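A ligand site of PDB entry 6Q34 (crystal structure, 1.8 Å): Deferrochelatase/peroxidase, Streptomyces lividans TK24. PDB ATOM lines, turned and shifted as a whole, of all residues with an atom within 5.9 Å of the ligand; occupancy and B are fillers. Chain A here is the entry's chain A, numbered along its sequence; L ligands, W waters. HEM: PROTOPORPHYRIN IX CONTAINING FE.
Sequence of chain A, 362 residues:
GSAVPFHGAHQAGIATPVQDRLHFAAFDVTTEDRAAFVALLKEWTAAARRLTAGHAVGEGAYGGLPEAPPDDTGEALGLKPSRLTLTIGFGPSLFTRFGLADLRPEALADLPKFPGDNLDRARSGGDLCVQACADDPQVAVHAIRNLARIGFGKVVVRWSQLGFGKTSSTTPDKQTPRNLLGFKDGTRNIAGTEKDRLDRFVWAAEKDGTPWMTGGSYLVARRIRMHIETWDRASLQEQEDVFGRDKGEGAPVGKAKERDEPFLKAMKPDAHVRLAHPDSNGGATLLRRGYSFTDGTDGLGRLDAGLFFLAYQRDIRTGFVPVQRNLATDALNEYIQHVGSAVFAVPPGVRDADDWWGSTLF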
ATOM      1  N   ASN A 179       7.553  19.960  21.128  1.00  0.00           N
ATOM      2  CA  ASN A 179       8.549  20.416  22.084  1.00  0.00           C
ATOM      3  C   ASN A 179       7.963  20.391  23.489  1.00  0.00           C
ATOM      4  O   ASN A 179       6.817  19.981  23.719  1.00  0.00           O
ATOM      5  CB  ASN A 179       9.058  21.799  21.681  1.00  0.00           C
ATOM      6  CG  ASN A 179       7.942  22.801  21.496  1.00  0.00           C
ATOM      7  OD1 ASN A 179       6.985  22.839  22.285  1.00  0.00           O
ATOM      8  ND2 ASN A 179       8.022  23.590  20.446  1.00  0.00           N
ATOM      9  N   LEU A 181       7.072  22.810  25.398  1.00  0.00           N
ATOM     10  CA  LEU A 181       5.878  23.650  25.555  1.00  0.00           C
ATOM     11  C   LEU A 181       4.611  22.991  25.049  1.00  0.00           C
ATOM     12  O   LEU A 181       3.541  23.609  25.133  1.00  0.00           O
ATOM     13  CB  LEU A 181       6.075  24.994  24.842  1.00  0.00           C
ATOM     14  CG  LEU A 181       7.377  25.710  25.169  1.00  0.00           C
ATOM     15  CD1 LEU A 181       7.443  27.010  24.384  1.00  0.00           C
ATOM     16  CD2 LEU A 181       7.451  25.941  26.637  1.00  0.00           C
ATOM     17  N   PHE A 183       3.762  22.036  21.823  1.00  0.00           N
ATOM     18  CA  PHE A 183       3.344  22.325  20.459  1.00  0.00           C
ATOM     19  C   PHE A 183       4.136  21.505  19.465  1.00  0.00           C
ATOM     20  O   PHE A 183       5.347  21.298  19.631  1.00  0.00           O
ATOM     21  CB  PHE A 183       3.515  23.805  20.133  1.00  0.00           C
ATOM     22  CG  PHE A 183       2.390  24.675  20.619  1.00  0.00           C
ATOM     23  CD1 PHE A 183       2.250  24.966  21.975  1.00  0.00           C
ATOM     24  CD2 PHE A 183       1.477  25.185  19.732  1.00  0.00           C
ATOM     25  CE1 PHE A 183       1.213  25.780  22.412  1.00  0.00           C
ATOM     26  CE2 PHE A 183       0.438  25.971  20.163  1.00  0.00           C
ATOM     27  CZ  PHE A 183       0.299  26.266  21.502  1.00  0.00           C
ATOM     28  N   LYS A 184       3.459  21.048  18.403  1.00  0.00           N
ATOM     29  CA  LYS A 184       4.169  20.447  17.273  1.00  0.00           C
ATOM     30  C   LYS A 184       5.214  21.430  16.765  1.00  0.00           C
ATOM     31  O   LYS A 184       4.983  22.630  16.733  1.00  0.00           O
ATOM     32  CB  LYS A 184       3.197  20.093  16.140  1.00  0.00           C
ATOM     33  CG  LYS A 184       2.055  19.151  16.538  1.00  0.00           C
ATOM     34  CD  LYS A 184       1.050  19.006  15.397  1.00  0.00           C
ATOM     35  CE  LYS A 184       0.147  17.775  15.614  1.00  0.00           C
ATOM     36  NZ  LYS A 184      -0.857  17.543  14.532  1.00  0.00           N
ATOM     37  N   ASP A 185       6.371  20.900  16.371  1.00  0.00           N
ATOM     38  CA  ASP A 185       7.540  21.709  16.037  1.00  0.00           C
ATOM     39  C   ASP A 185       8.200  21.068  14.816  1.00  0.00           C
ATOM     40  O   ASP A 185       8.728  19.958  14.930  1.00  0.00           O
ATOM     41  CB  ASP A 185       8.515  21.739  17.222  1.00  0.00           C
ATOM     42  CG  ASP A 185       9.409  22.967  17.253  1.00  0.00           C
ATOM     43  OD1 ASP A 185       9.698  23.576  16.202  1.00  0.00           O
ATOM     44  OD2 ASP A 185       9.847  23.333  18.375  1.00  0.00           O
ATOM     45  N   GLY A 186       8.211  21.766  13.681  1.00  0.00           N
ATOM     46  CA  GLY A 186       8.779  21.239  12.443  1.00  0.00           C
ATOM     47  C   GLY A 186       7.814  21.188  11.255  1.00  0.00           C
ATOM     48  O   GLY A 186       8.252  20.850  10.143  1.00  0.00           O
ATOM     49  N   THR A 187       6.544  21.548  11.441  1.00  0.00           N
ATOM     50  CA  THR A 187       5.553  21.503  10.370  1.00  0.00           C
ATOM     51  C   THR A 187       6.071  22.174   9.096  1.00  0.00           C
ATOM     52  O   THR A 187       6.114  21.554   8.023  1.00  0.00           O
ATOM     53  CB  THR A 187       4.272  22.170  10.855  1.00  0.00           C
ATOM     54  OG1 THR A 187       3.782  21.438  11.994  1.00  0.00           O
ATOM     55  CG2 THR A 187       3.178  22.225   9.769  1.00  0.00           C
ATOM     56  N   ARG A 188       6.493  23.436   9.187  1.00  0.00           N
ATOM     57  CA  ARG A 188       6.921  24.194   8.023  1.00  0.00           C
ATOM     58  C   ARG A 188       8.440  24.357   8.057  1.00  0.00           C
ATOM     59  O   ARG A 188       8.992  25.430   8.289  1.00  0.00           O
ATOM     60  CB  ARG A 188       6.149  25.555   7.933  1.00  0.00           C
ATOM     61  CG  ARG A 188       4.771  25.390   7.250  1.00  0.00           C
ATOM     62  CD  ARG A 188       4.063  26.731   6.926  1.00  0.00           C
ATOM     63  NE  ARG A 188       5.054  27.763   6.612  1.00  0.00           N
ATOM     64  CZ  ARG A 188       5.615  27.935   5.412  1.00  0.00           C
ATOM     65  NH1 ARG A 188       6.530  28.878   5.243  1.00  0.00           N
ATOM     66  NH2 ARG A 188       5.235  27.188   4.377  1.00  0.00           N
ATOM     67  N   ASN A 189       9.115  23.241   7.801  1.00  0.00           N
ATOM     68  CA  ASN A 189      10.568  23.140   7.708  1.00  0.00           C
ATOM     69  C   ASN A 189      10.904  22.651   6.303  1.00  0.00           C
ATOM     70  O   ASN A 189      10.029  22.220   5.545  1.00  0.00           O
ATOM     71  CB  ASN A 189      11.114  22.175   8.780  1.00  0.00           C
ATOM     72  CG  ASN A 189      12.593  22.345   9.030  1.00  0.00           C
ATOM     73  OD1 ASN A 189      13.088  23.451   9.204  1.00  0.00           O
ATOM     74  ND2 ASN A 189      13.313  21.226   9.099  1.00  0.00           N
ATOM     75  N   ILE A 224      18.585  27.326  24.399  1.00  0.00           N
ATOM     76  CA  ILE A 224      17.474  28.172  24.787  1.00  0.00           C
ATOM     77  C   ILE A 224      16.780  27.576  25.996  1.00  0.00           C
ATOM     78  O   ILE A 224      16.170  26.500  25.905  1.00  0.00           O
ATOM     79  CB  ILE A 224      16.481  28.368  23.641  1.00  0.00           C
ATOM     80  CG1 ILE A 224      17.201  28.859  22.371  1.00  0.00           C
ATOM     81  CG2 ILE A 224      15.385  29.342  24.039  1.00  0.00           C
ATOM     82  CD1 ILE A 224      16.298  28.967  21.157  1.00  0.00           C
ATOM     83  N   MET A 226      13.760  27.394  28.718  1.00  0.00           N
ATOM     84  CA  MET A 226      12.324  27.667  28.748  1.00  0.00           C
ATOM     85  C   MET A 226      11.848  27.925  30.177  1.00  0.00           C
ATOM     86  O   MET A 226      12.181  27.180  31.105  1.00  0.00           O
ATOM     87  CB  MET A 226      11.540  26.485  28.158  1.00  0.00           C
ATOM     88  CG  MET A 226      11.762  26.312  26.688  1.00  0.00           C
ATOM     89  SD  MET A 226      11.063  24.725  26.213  1.00  0.00           S
ATOM     90  CE  MET A 226      11.143  24.901  24.444  1.00  0.00           C
ATOM     91  N   PHE A 243       1.920  31.539  19.471  1.00  0.00           N
ATOM     92  CA  PHE A 243       2.460  30.911  18.280  1.00  0.00           C
ATOM     93  C   PHE A 243       1.721  31.271  17.001  1.00  0.00           C
ATOM     94  O   PHE A 243       2.372  31.499  15.966  1.00  0.00           O
ATOM     95  CB  PHE A 243       2.481  29.391  18.436  1.00  0.00           C
ATOM     96  CG  PHE A 243       3.568  28.928  19.329  1.00  0.00           C
ATOM     97  CD1 PHE A 243       4.894  29.075  18.958  1.00  0.00           C
ATOM     98  CD2 PHE A 243       3.275  28.425  20.562  1.00  0.00           C
ATOM     99  CE1 PHE A 243       5.926  28.683  19.819  1.00  0.00           C
ATOM    100  CE2 PHE A 243       4.292  28.046  21.435  1.00  0.00           C
ATOM    101  CZ  PHE A 243       5.611  28.160  21.051  1.00  0.00           C
ATOM    102  N   ARG A 245      -0.793  29.060  16.108  1.00  0.00           N
ATOM    103  CA  ARG A 245      -1.362  27.776  15.753  1.00  0.00           C
ATOM    104  C   ARG A 245      -2.050  27.223  16.996  1.00  0.00           C
ATOM    105  O   ARG A 245      -1.662  27.518  18.127  1.00  0.00           O
ATOM    106  CB  ARG A 245      -0.287  26.790  15.255  1.00  0.00           C
ATOM    107  CG  ARG A 245       0.404  27.146  13.948  1.00  0.00           C
ATOM    108  CD  ARG A 245       1.532  26.151  13.667  1.00  0.00           C
ATOM    109  NE  ARG A 245       2.186  26.335  12.368  1.00  0.00           N
ATOM    110  CZ  ARG A 245       1.756  25.790  11.233  1.00  0.00           C
ATOM    111  NH1 ARG A 245       0.666  25.033  11.260  1.00  0.00           N
ATOM    112  NH2 ARG A 245       2.406  25.997  10.092  1.00  0.00           N
ATOM    113  N   PRO A 262      -0.562  28.794   6.627  1.00  0.00           N
ATOM    114  CA  PRO A 262      -0.929  29.890   7.531  1.00  0.00           C
ATOM    115  C   PRO A 262      -1.396  31.107   6.735  1.00  0.00           C
ATOM    116  O   PRO A 262      -0.905  31.393   5.639  1.00  0.00           O
ATOM    117  CB  PRO A 262       0.377  30.194   8.277  1.00  0.00           C
ATOM    118  CG  PRO A 262       1.443  29.662   7.374  1.00  0.00           C
ATOM    119  CD  PRO A 262       0.861  28.448   6.735  1.00  0.00           C
ATOM    120  N   HIS A 272       4.657  34.200  16.882  1.00  0.00           N
ATOM    121  CA  HIS A 272       5.953  33.645  16.510  1.00  0.00           C
ATOM    122  C   HIS A 272       5.988  33.214  15.042  1.00  0.00           C
ATOM    123  O   HIS A 272       6.895  33.598  14.305  1.00  0.00           O
ATOM    124  CB  HIS A 272       6.277  32.477  17.443  1.00  0.00           C
ATOM    125  CG  HIS A 272       7.578  31.815  17.157  1.00  0.00           C
ATOM    126  ND1 HIS A 272       8.791  32.401  17.423  1.00  0.00           N
ATOM    127  CD2 HIS A 272       7.852  30.594  16.632  1.00  0.00           C
ATOM    128  CE1 HIS A 272       9.763  31.577  17.095  1.00  0.00           C
ATOM    129  NE2 HIS A 272       9.223  30.474  16.597  1.00  0.00           N
ATOM    130  N   VAL A 273       4.988  32.450  14.598  1.00  0.00           N
ATOM    131  CA  VAL A 273       5.001  31.974  13.213  1.00  0.00           C
ATOM    132  C   VAL A 273       4.904  33.153  12.254  1.00  0.00           C
ATOM    133  O   VAL A 273       5.574  33.179  11.202  1.00  0.00           O
ATOM    134  CB  VAL A 273       3.855  30.962  12.967  1.00  0.00           C
ATOM    135  CG1 VAL A 273       3.659  30.721  11.465  1.00  0.00           C
ATOM    136  CG2 VAL A 273       4.169  29.661  13.652  1.00  0.00           C
ATOM    137  N   ALA A 276       8.441  34.693  12.163  1.00  0.00           N
ATOM    138  CA  ALA A 276       9.490  33.842  11.625  1.00  0.00           C
ATOM    139  C   ALA A 276       9.261  33.432  10.179  1.00  0.00           C
ATOM    140  O   ALA A 276      10.195  32.958   9.534  1.00  0.00           O
ATOM    141  CB  ALA A 276       9.658  32.574  12.460  1.00  0.00           C
ATOM    142  N   HIS A 277       8.050  33.621   9.665  1.00  0.00           N
ATOM    143  CA  HIS A 277       7.679  33.068   8.369  1.00  0.00           C
ATOM    144  C   HIS A 277       8.517  33.713   7.275  1.00  0.00           C
ATOM    145  O   HIS A 277       8.834  34.892   7.360  1.00  0.00           O
ATOM    146  CB  HIS A 277       6.187  33.325   8.134  1.00  0.00           C
ATOM    147  CG  HIS A 277       5.591  32.563   7.000  1.00  0.00           C
ATOM    148  ND1 HIS A 277       5.688  32.981   5.680  1.00  0.00           N
ATOM    149  CD2 HIS A 277       4.825  31.437   6.976  1.00  0.00           C
ATOM    150  CE1 HIS A 277       5.042  32.132   4.902  1.00  0.00           C
ATOM    151  NE2 HIS A 277       4.505  31.197   5.661  1.00  0.00           N
ATOM    152  N   PRO A 278       8.913  32.964   6.233  1.00  0.00           N
ATOM    153  CA  PRO A 278       9.756  33.575   5.186  1.00  0.00           C
ATOM    154  C   PRO A 278       9.159  34.856   4.589  1.00  0.00           C
ATOM    155  O   PRO A 278       9.907  35.804   4.307  1.00  0.00           O
ATOM    156  CB  PRO A 278       9.873  32.454   4.141  1.00  0.00           C
ATOM    157  CG  PRO A 278       9.775  31.207   4.933  1.00  0.00           C
ATOM    158  CD  PRO A 278       8.790  31.503   6.052  1.00  0.00           C
ATOM    159  N   LEU A 286      14.993  28.632   6.735  1.00  0.00           N
ATOM    160  CA  LEU A 286      15.901  27.877   7.583  1.00  0.00           C
ATOM    161  C   LEU A 286      15.550  26.397   7.527  1.00  0.00           C
ATOM    162  O   LEU A 286      14.398  26.027   7.277  1.00  0.00           O
ATOM    163  CB  LEU A 286      15.814  28.345   9.041  1.00  0.00           C
ATOM    164  CG  LEU A 286      16.286  29.762   9.330  1.00  0.00           C
ATOM    165  CD1 LEU A 286      15.974  30.150  10.752  1.00  0.00           C
ATOM    166  CD2 LEU A 286      17.784  29.853   9.038  1.00  0.00           C
ATOM    167  N   ARG A 288      15.535  23.788  10.347  1.00  0.00           N
ATOM    168  CA  ARG A 288      15.624  23.560  11.781  1.00  0.00           C
ATOM    169  C   ARG A 288      15.807  22.077  12.063  1.00  0.00           C
ATOM    170  O   ARG A 288      15.157  21.237  11.441  1.00  0.00           O
ATOM    171  CB  ARG A 288      14.379  24.109  12.490  1.00  0.00           C
ATOM    172  CG  ARG A 288      14.268  25.642  12.481  1.00  0.00           C
ATOM    173  CD  ARG A 288      12.876  26.157  12.946  1.00  0.00           C
ATOM    174  NE  ARG A 288      11.837  25.824  11.982  1.00  0.00           N
ATOM    175  CZ  ARG A 288      10.641  25.353  12.282  1.00  0.00           C
ATOM    176  NH1 ARG A 288      10.283  25.167  13.555  1.00  0.00           N
ATOM    177  NH2 ARG A 288       9.785  25.056  11.298  1.00  0.00           N
ATOM    178  N   LEU A 307      15.428  23.989  24.883  1.00  0.00           N
ATOM    179  CA  LEU A 307      15.555  23.512  23.517  1.00  0.00           C
ATOM    180  C   LEU A 307      16.941  23.846  22.996  1.00  0.00           C
ATOM    181  O   LEU A 307      17.387  24.997  23.084  1.00  0.00           O
ATOM    182  CB  LEU A 307      14.490  24.161  22.629  1.00  0.00           C
ATOM    183  CG  LEU A 307      14.401  23.631  21.204  1.00  0.00           C
ATOM    184  CD1 LEU A 307      12.945  23.438  20.850  1.00  0.00           C
ATOM    185  CD2 LEU A 307      15.064  24.616  20.261  1.00  0.00           C
ATOM    186  N   PHE A 309      18.686  24.527  19.966  1.00  0.00           N
ATOM    187  CA  PHE A 309      18.213  24.905  18.650  1.00  0.00           C
ATOM    188  C   PHE A 309      19.364  24.857  17.655  1.00  0.00           C
ATOM    189  O   PHE A 309      20.437  25.419  17.894  1.00  0.00           O
ATOM    190  CB  PHE A 309      17.570  26.304  18.731  1.00  0.00           C
ATOM    191  CG  PHE A 309      17.098  26.866  17.406  1.00  0.00           C
ATOM    192  CD1 PHE A 309      17.972  27.617  16.605  1.00  0.00           C
ATOM    193  CD2 PHE A 309      15.771  26.698  16.977  1.00  0.00           C
ATOM    194  CE1 PHE A 309      17.550  28.158  15.388  1.00  0.00           C
ATOM    195  CE2 PHE A 309      15.334  27.242  15.753  1.00  0.00           C
ATOM    196  CZ  PHE A 309      16.237  27.973  14.963  1.00  0.00           C
ATOM    197  N   PHE A 320      19.821  32.825   9.526  1.00  0.00           N
ATOM    198  CA  PHE A 320      19.470  32.981  10.930  1.00  0.00           C
ATOM    199  C   PHE A 320      19.382  34.452  11.327  1.00  0.00           C
ATOM    200  O   PHE A 320      18.473  34.836  12.075  1.00  0.00           O
ATOM    201  CB  PHE A 320      20.489  32.243  11.812  1.00  0.00           C
ATOM    202  CG  PHE A 320      20.272  32.447  13.272  1.00  0.00           C
ATOM    203  CD1 PHE A 320      19.311  31.715  13.960  1.00  0.00           C
ATOM    204  CD2 PHE A 320      21.024  33.375  13.977  1.00  0.00           C
ATOM    205  CE1 PHE A 320      19.109  31.909  15.324  1.00  0.00           C
ATOM    206  CE2 PHE A 320      20.831  33.569  15.337  1.00  0.00           C
ATOM    207  CZ  PHE A 320      19.870  32.848  16.003  1.00  0.00           C
ATOM    208  N   VAL A 323      16.007  36.463  10.370  1.00  0.00           N
ATOM    209  CA  VAL A 323      14.859  35.905  11.079  1.00  0.00           C
ATOM    210  C   VAL A 323      14.962  36.198  12.582  1.00  0.00           C
ATOM    211  O   VAL A 323      13.989  36.620  13.218  1.00  0.00           O
ATOM    212  CB  VAL A 323      14.704  34.407  10.780  1.00  0.00           C
ATOM    213  CG1 VAL A 323      13.428  33.856  11.446  1.00  0.00           C
ATOM    214  CG2 VAL A 323      14.648  34.168   9.241  1.00  0.00           C
ATOM    215  N   GLN A 324      16.151  36.012  13.159  1.00  0.00           N
ATOM    216  CA  GLN A 324      16.295  36.281  14.590  1.00  0.00           C
ATOM    217  C   GLN A 324      16.100  37.767  14.900  1.00  0.00           C
ATOM    218  O   GLN A 324      15.505  38.122  15.939  1.00  0.00           O
ATOM    219  CB  GLN A 324      17.671  35.791  15.078  1.00  0.00           C
ATOM    220  CG  GLN A 324      17.989  36.069  16.554  1.00  0.00           C
ATOM    221  CD  GLN A 324      16.908  35.567  17.507  1.00  0.00           C
ATOM    222  OE1 GLN A 324      16.665  34.360  17.615  1.00  0.00           O
ATOM    223  NE2 GLN A 324      16.272  36.498  18.192  1.00  0.00           N
ATOM    224  N   LEU A 327      12.579  38.639  15.328  1.00  0.00           N
ATOM    225  CA  LEU A 327      11.930  38.129  16.519  1.00  0.00           C
ATOM    226  C   LEU A 327      12.136  39.012  17.740  1.00  0.00           C
ATOM    227  O   LEU A 327      11.723  38.628  18.848  1.00  0.00           O
ATOM    228  CB  LEU A 327      12.407  36.701  16.816  1.00  0.00           C
ATOM    229  CG  LEU A 327      12.270  35.654  15.711  1.00  0.00           C
ATOM    230  CD1 LEU A 327      12.742  34.292  16.206  1.00  0.00           C
ATOM    231  CD2 LEU A 327      10.839  35.587  15.202  1.00  0.00           C
ATOM    232  N   LEU A 332       6.904  35.039  22.099  1.00  0.00           N
ATOM    233  CA  LEU A 332       7.557  33.896  22.743  1.00  0.00           C
ATOM    234  C   LEU A 332       8.674  34.349  23.688  1.00  0.00           C
ATOM    235  O   LEU A 332       9.005  33.637  24.634  1.00  0.00           O
ATOM    236  CB  LEU A 332       8.102  32.931  21.691  1.00  0.00           C
ATOM    237  CG  LEU A 332       8.737  31.614  22.171  1.00  0.00           C
ATOM    238  CD1 LEU A 332       7.720  30.811  22.939  1.00  0.00           C
ATOM    239  CD2 LEU A 332       9.285  30.815  20.988  1.00  0.00           C
ATOM    240  N   ILE A 336      11.261  32.455  27.023  1.00  0.00           N
ATOM    241  CA  ILE A 336      12.481  31.784  26.613  1.00  0.00           C
ATOM    242  C   ILE A 336      13.658  32.716  26.911  1.00  0.00           C
ATOM    243  O   ILE A 336      13.510  33.926  27.027  1.00  0.00           O
ATOM    244  CB  ILE A 336      12.473  31.394  25.113  1.00  0.00           C
ATOM    245  CG1 ILE A 336      12.415  32.658  24.248  1.00  0.00           C
ATOM    246  CG2 ILE A 336      11.289  30.466  24.804  1.00  0.00           C
ATOM    247  CD1 ILE A 336      13.075  32.480  22.904  1.00  0.00           C
ATOM    248  N   HIS A 338      17.918  32.907  25.578  1.00  0.00           N
ATOM    249  CA  HIS A 338      19.064  32.292  24.916  1.00  0.00           C
ATOM    250  C   HIS A 338      20.257  32.346  25.857  1.00  0.00           C
ATOM    251  O   HIS A 338      20.643  33.432  26.305  1.00  0.00           O
ATOM    252  CB  HIS A 338      19.381  33.002  23.592  1.00  0.00           C
ATOM    253  CG  HIS A 338      18.337  32.823  22.522  1.00  0.00           C
ATOM    254  ND1 HIS A 338      18.604  32.242  21.299  1.00  0.00           N
ATOM    255  CD2 HIS A 338      17.021  33.167  22.504  1.00  0.00           C
ATOM    256  CE1 HIS A 338      17.499  32.226  20.577  1.00  0.00           C
ATOM    257  NE2 HIS A 338      16.527  32.778  21.281  1.00  0.00           N
HETATM  258  CHA HEM L   1       7.919  27.614  13.641  1.00  0.00           C
HETATM  259  CHB HEM L   1       8.531  26.830  18.371  1.00  0.00           C
HETATM  260  CHC HEM L   1      12.728  29.214  18.347  1.00  0.00           C
HETATM  261  CHD HEM L   1      12.232  29.908  13.575  1.00  0.00           C
HETATM  262  C1A HEM L   1       7.686  27.203  14.923  1.00  0.00           C
HETATM  263  C2A HEM L   1       6.512  26.513  15.418  1.00  0.00           C
HETATM  264  C3A HEM L   1       6.693  26.309  16.731  1.00  0.00           C
HETATM  265  C4A HEM L   1       7.983  26.862  17.111  1.00  0.00           C
HETATM  266  CMA HEM L   1       5.715  25.622  17.717  1.00  0.00           C
HETATM  267  CAA HEM L   1       5.295  26.134  14.542  1.00  0.00           C
HETATM  268  CBA HEM L   1       5.449  24.821  13.759  1.00  0.00           C
HETATM  269  CGA HEM L   1       6.494  24.800  12.657  1.00  0.00           C
HETATM  270  O1A HEM L   1       7.629  24.339  12.921  1.00  0.00           O
HETATM  271  O2A HEM L   1       6.174  25.212  11.514  1.00  0.00           O
HETATM  272  C1B HEM L   1       9.721  27.378  18.757  1.00  0.00           C
HETATM  273  C2B HEM L   1      10.265  27.323  20.089  1.00  0.00           C
HETATM  274  C3B HEM L   1      11.428  27.997  20.106  1.00  0.00           C
HETATM  275  C4B HEM L   1      11.647  28.488  18.761  1.00  0.00           C
HETATM  276  CMB HEM L   1       9.567  26.603  21.266  1.00  0.00           C
HETATM  277  CAB HEM L   1      12.410  28.206  21.269  1.00  0.00           C
HETATM  278  CBB HEM L   1      12.320  27.483  22.385  1.00  0.00           C
HETATM  279  C1C HEM L   1      12.945  29.628  17.057  1.00  0.00           C
HETATM  280  C2C HEM L   1      14.079  30.405  16.618  1.00  0.00           C
HETATM  281  C3C HEM L   1      13.946  30.579  15.286  1.00  0.00           C
HETATM  282  C4C HEM L   1      12.719  29.947  14.873  1.00  0.00           C
HETATM  283  CMC HEM L   1      15.185  30.855  17.584  1.00  0.00           C
HETATM  284  CAC HEM L   1      14.851  31.347  14.296  1.00  0.00           C
HETATM  285  CBC HEM L   1      15.826  32.149  14.740  1.00  0.00           C
HETATM  286  C1D HEM L   1      11.051  29.315  13.164  1.00  0.00           C
HETATM  287  C2D HEM L   1      10.575  29.188  11.801  1.00  0.00           C
HETATM  288  C3D HEM L   1       9.385  28.559  11.820  1.00  0.00           C
HETATM  289  C4D HEM L   1       9.063  28.261  13.193  1.00  0.00           C
HETATM  290  CMD HEM L   1      11.301  29.697  10.542  1.00  0.00           C
HETATM  291  CAD HEM L   1       8.544  28.236  10.554  1.00  0.00           C
HETATM  292  CBD HEM L   1       7.509  29.341  10.292  1.00  0.00           C
HETATM  293  CGD HEM L   1       6.864  29.159   8.953  1.00  0.00           C
HETATM  294  O1D HEM L   1       7.578  29.257   7.921  1.00  0.00           O
HETATM  295  O2D HEM L   1       5.623  28.933   8.919  1.00  0.00           O
HETATM  296  NA  HEM L   1       8.547  27.407  15.995  1.00  0.00           N
HETATM  297  NB  HEM L   1      10.573  28.097  17.977  1.00  0.00           N
HETATM  298  NC  HEM L   1      12.148  29.369  15.975  1.00  0.00           N
HETATM  299  ND  HEM L   1      10.095  28.727  13.989  1.00  0.00           N
HETATM  300 FE   HEM L   1      10.246  28.544  15.985  1.00  0.00          FE
HETATM  301  O   HOH W   1       4.581  27.414  11.043  1.00  0.00           O
HETATM  302  O   HOH W   2       9.757  27.815   6.979  1.00  0.00           O
HETATM  303  O   HOH W   3      12.090  28.846   7.500  1.00  0.00           O
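The side-chain carboxylate (OD2) of Asp 185 lies within hydrogen-bond range of the side-chain amide nitrogen (ND2) of Asn 179 (2.8 Å). The guanidinium group (NH1) of Arg 288 is in salt-bridge range of the side-chain carboxylate (OD1) of Asp 185. O of Ile 224 is in hydrogen-bond range of N of Leu 307, at 2.8 Å. The backbone carbonyl oxygen (O) of Leu 286 lies close to the side-chain amide oxygen (OD1) of Asn 189. The backbone carbonyl oxygen (O) of Arg 188 is in hydrogen-bond range of the guanidinium group (NH2) of Arg 288. The backbone NH (N) of Leu 181 is in hydrogen-bond range of the side-chain amide oxygen (OD1) of Asn 179, at 3.1 Å. N of Arg 288 is in hydrogen-bond range of OD1 of Asn 189, at 2.7 Å. N of Phe 183 is in hydrogen-bond range of OD1 of Asn 179, at 3.4 Å.
Asn 179 touches the ligand. Leu 181 touches the ligand (CD1 to CMB, 3.8 Å). CB of Phe 183 touches CMA of the ligand, 3.7 Å away. O of Lys 184 touches CMA of the ligand, 3.2 Å away. Asp 185 touches the ligand (OD2 to CHB, 3.7 Å). Ile 224 touches the ligand (CG2 to CBB, 3.9 Å). CE of Met 226 touches CBB of the ligand, at 3.5 Å. Phe 243 touches the ligand. Arg 245 touches the ligand (NE to CAA, 3.8 Å). CG1 of Val 273 touches O2D of the ligand, at 3.7 Å. Ala 276 touches the ligand. His 277 touches the ligand. CD of Pro 278 touches O1D of the ligand (3.2 Å). Leu 286 touches the ligand. Leu 307 touches the ligand (CB to CBB, 3.98 Å). Phe 309 touches the ligand (CZ to C3C, 3.5 Å). Phe 320 touches the ligand. Gln 324 touches the ligand (OE1 to CBC, 3.7 Å). Leu 332 touches the ligand. Ile 336 touches the ligand (CG2 to CBB, 3.98 Å). Hydrophobic or aromatic side chains within 4 Å of the ligand: Leu 181, Phe 183, Ile 224, Met 226, Phe 243, His 272, Val 273, Ala 276, His 277, Pro 278, Leu 286, Leu 307, Phe 309, Phe 320, Leu 332 and Ile 336. Within 4 Å of the ligand: Asn 179, Leu 181, Phe 183, Lys 184, Asp 185, Gly 186, Thr 187, Arg 188, Ile 224, Met 226, Phe 243, Arg 245, His 272, Val 273, Ala 276, His 277, Pro 278, Leu 286, Arg 288, Leu 307, Phe 309, Phe 320, Gln 324, Leu 332 and Ile 336. The nearest printed residue that does not touch the ligand is Leu 327 (4.01 Å).
N of Gly 186 sits at hydrogen-bond distance from O1A of the ligand (2.7 Å). The guanidinium group (NH2) of Arg 288 is in salt-bridge range of an oxygen (O1A) of the ligand (2.8 Å). The guanidinium group (NE) of Arg 188 is in salt-bridge range of an oxygen (O2D) of the ligand. An iron atom (FE) of the ligand is bound by a ring nitrogen (NE2) of His 272 (2.3 Å). N of Thr 187 is in hydrogen-bond range of O1A of the ligand (3.3 Å). O2A of the ligand lies within hydrogen-bond range of N of Arg 188 (2.9 Å).
Water W1 bridges an oxygen (O2A) of the ligand and the guanidinium group (NH2) of Arg 245. Water W2 bridges O1D of the ligand (2.8 Å) and O of Arg 188 (2.8 Å).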
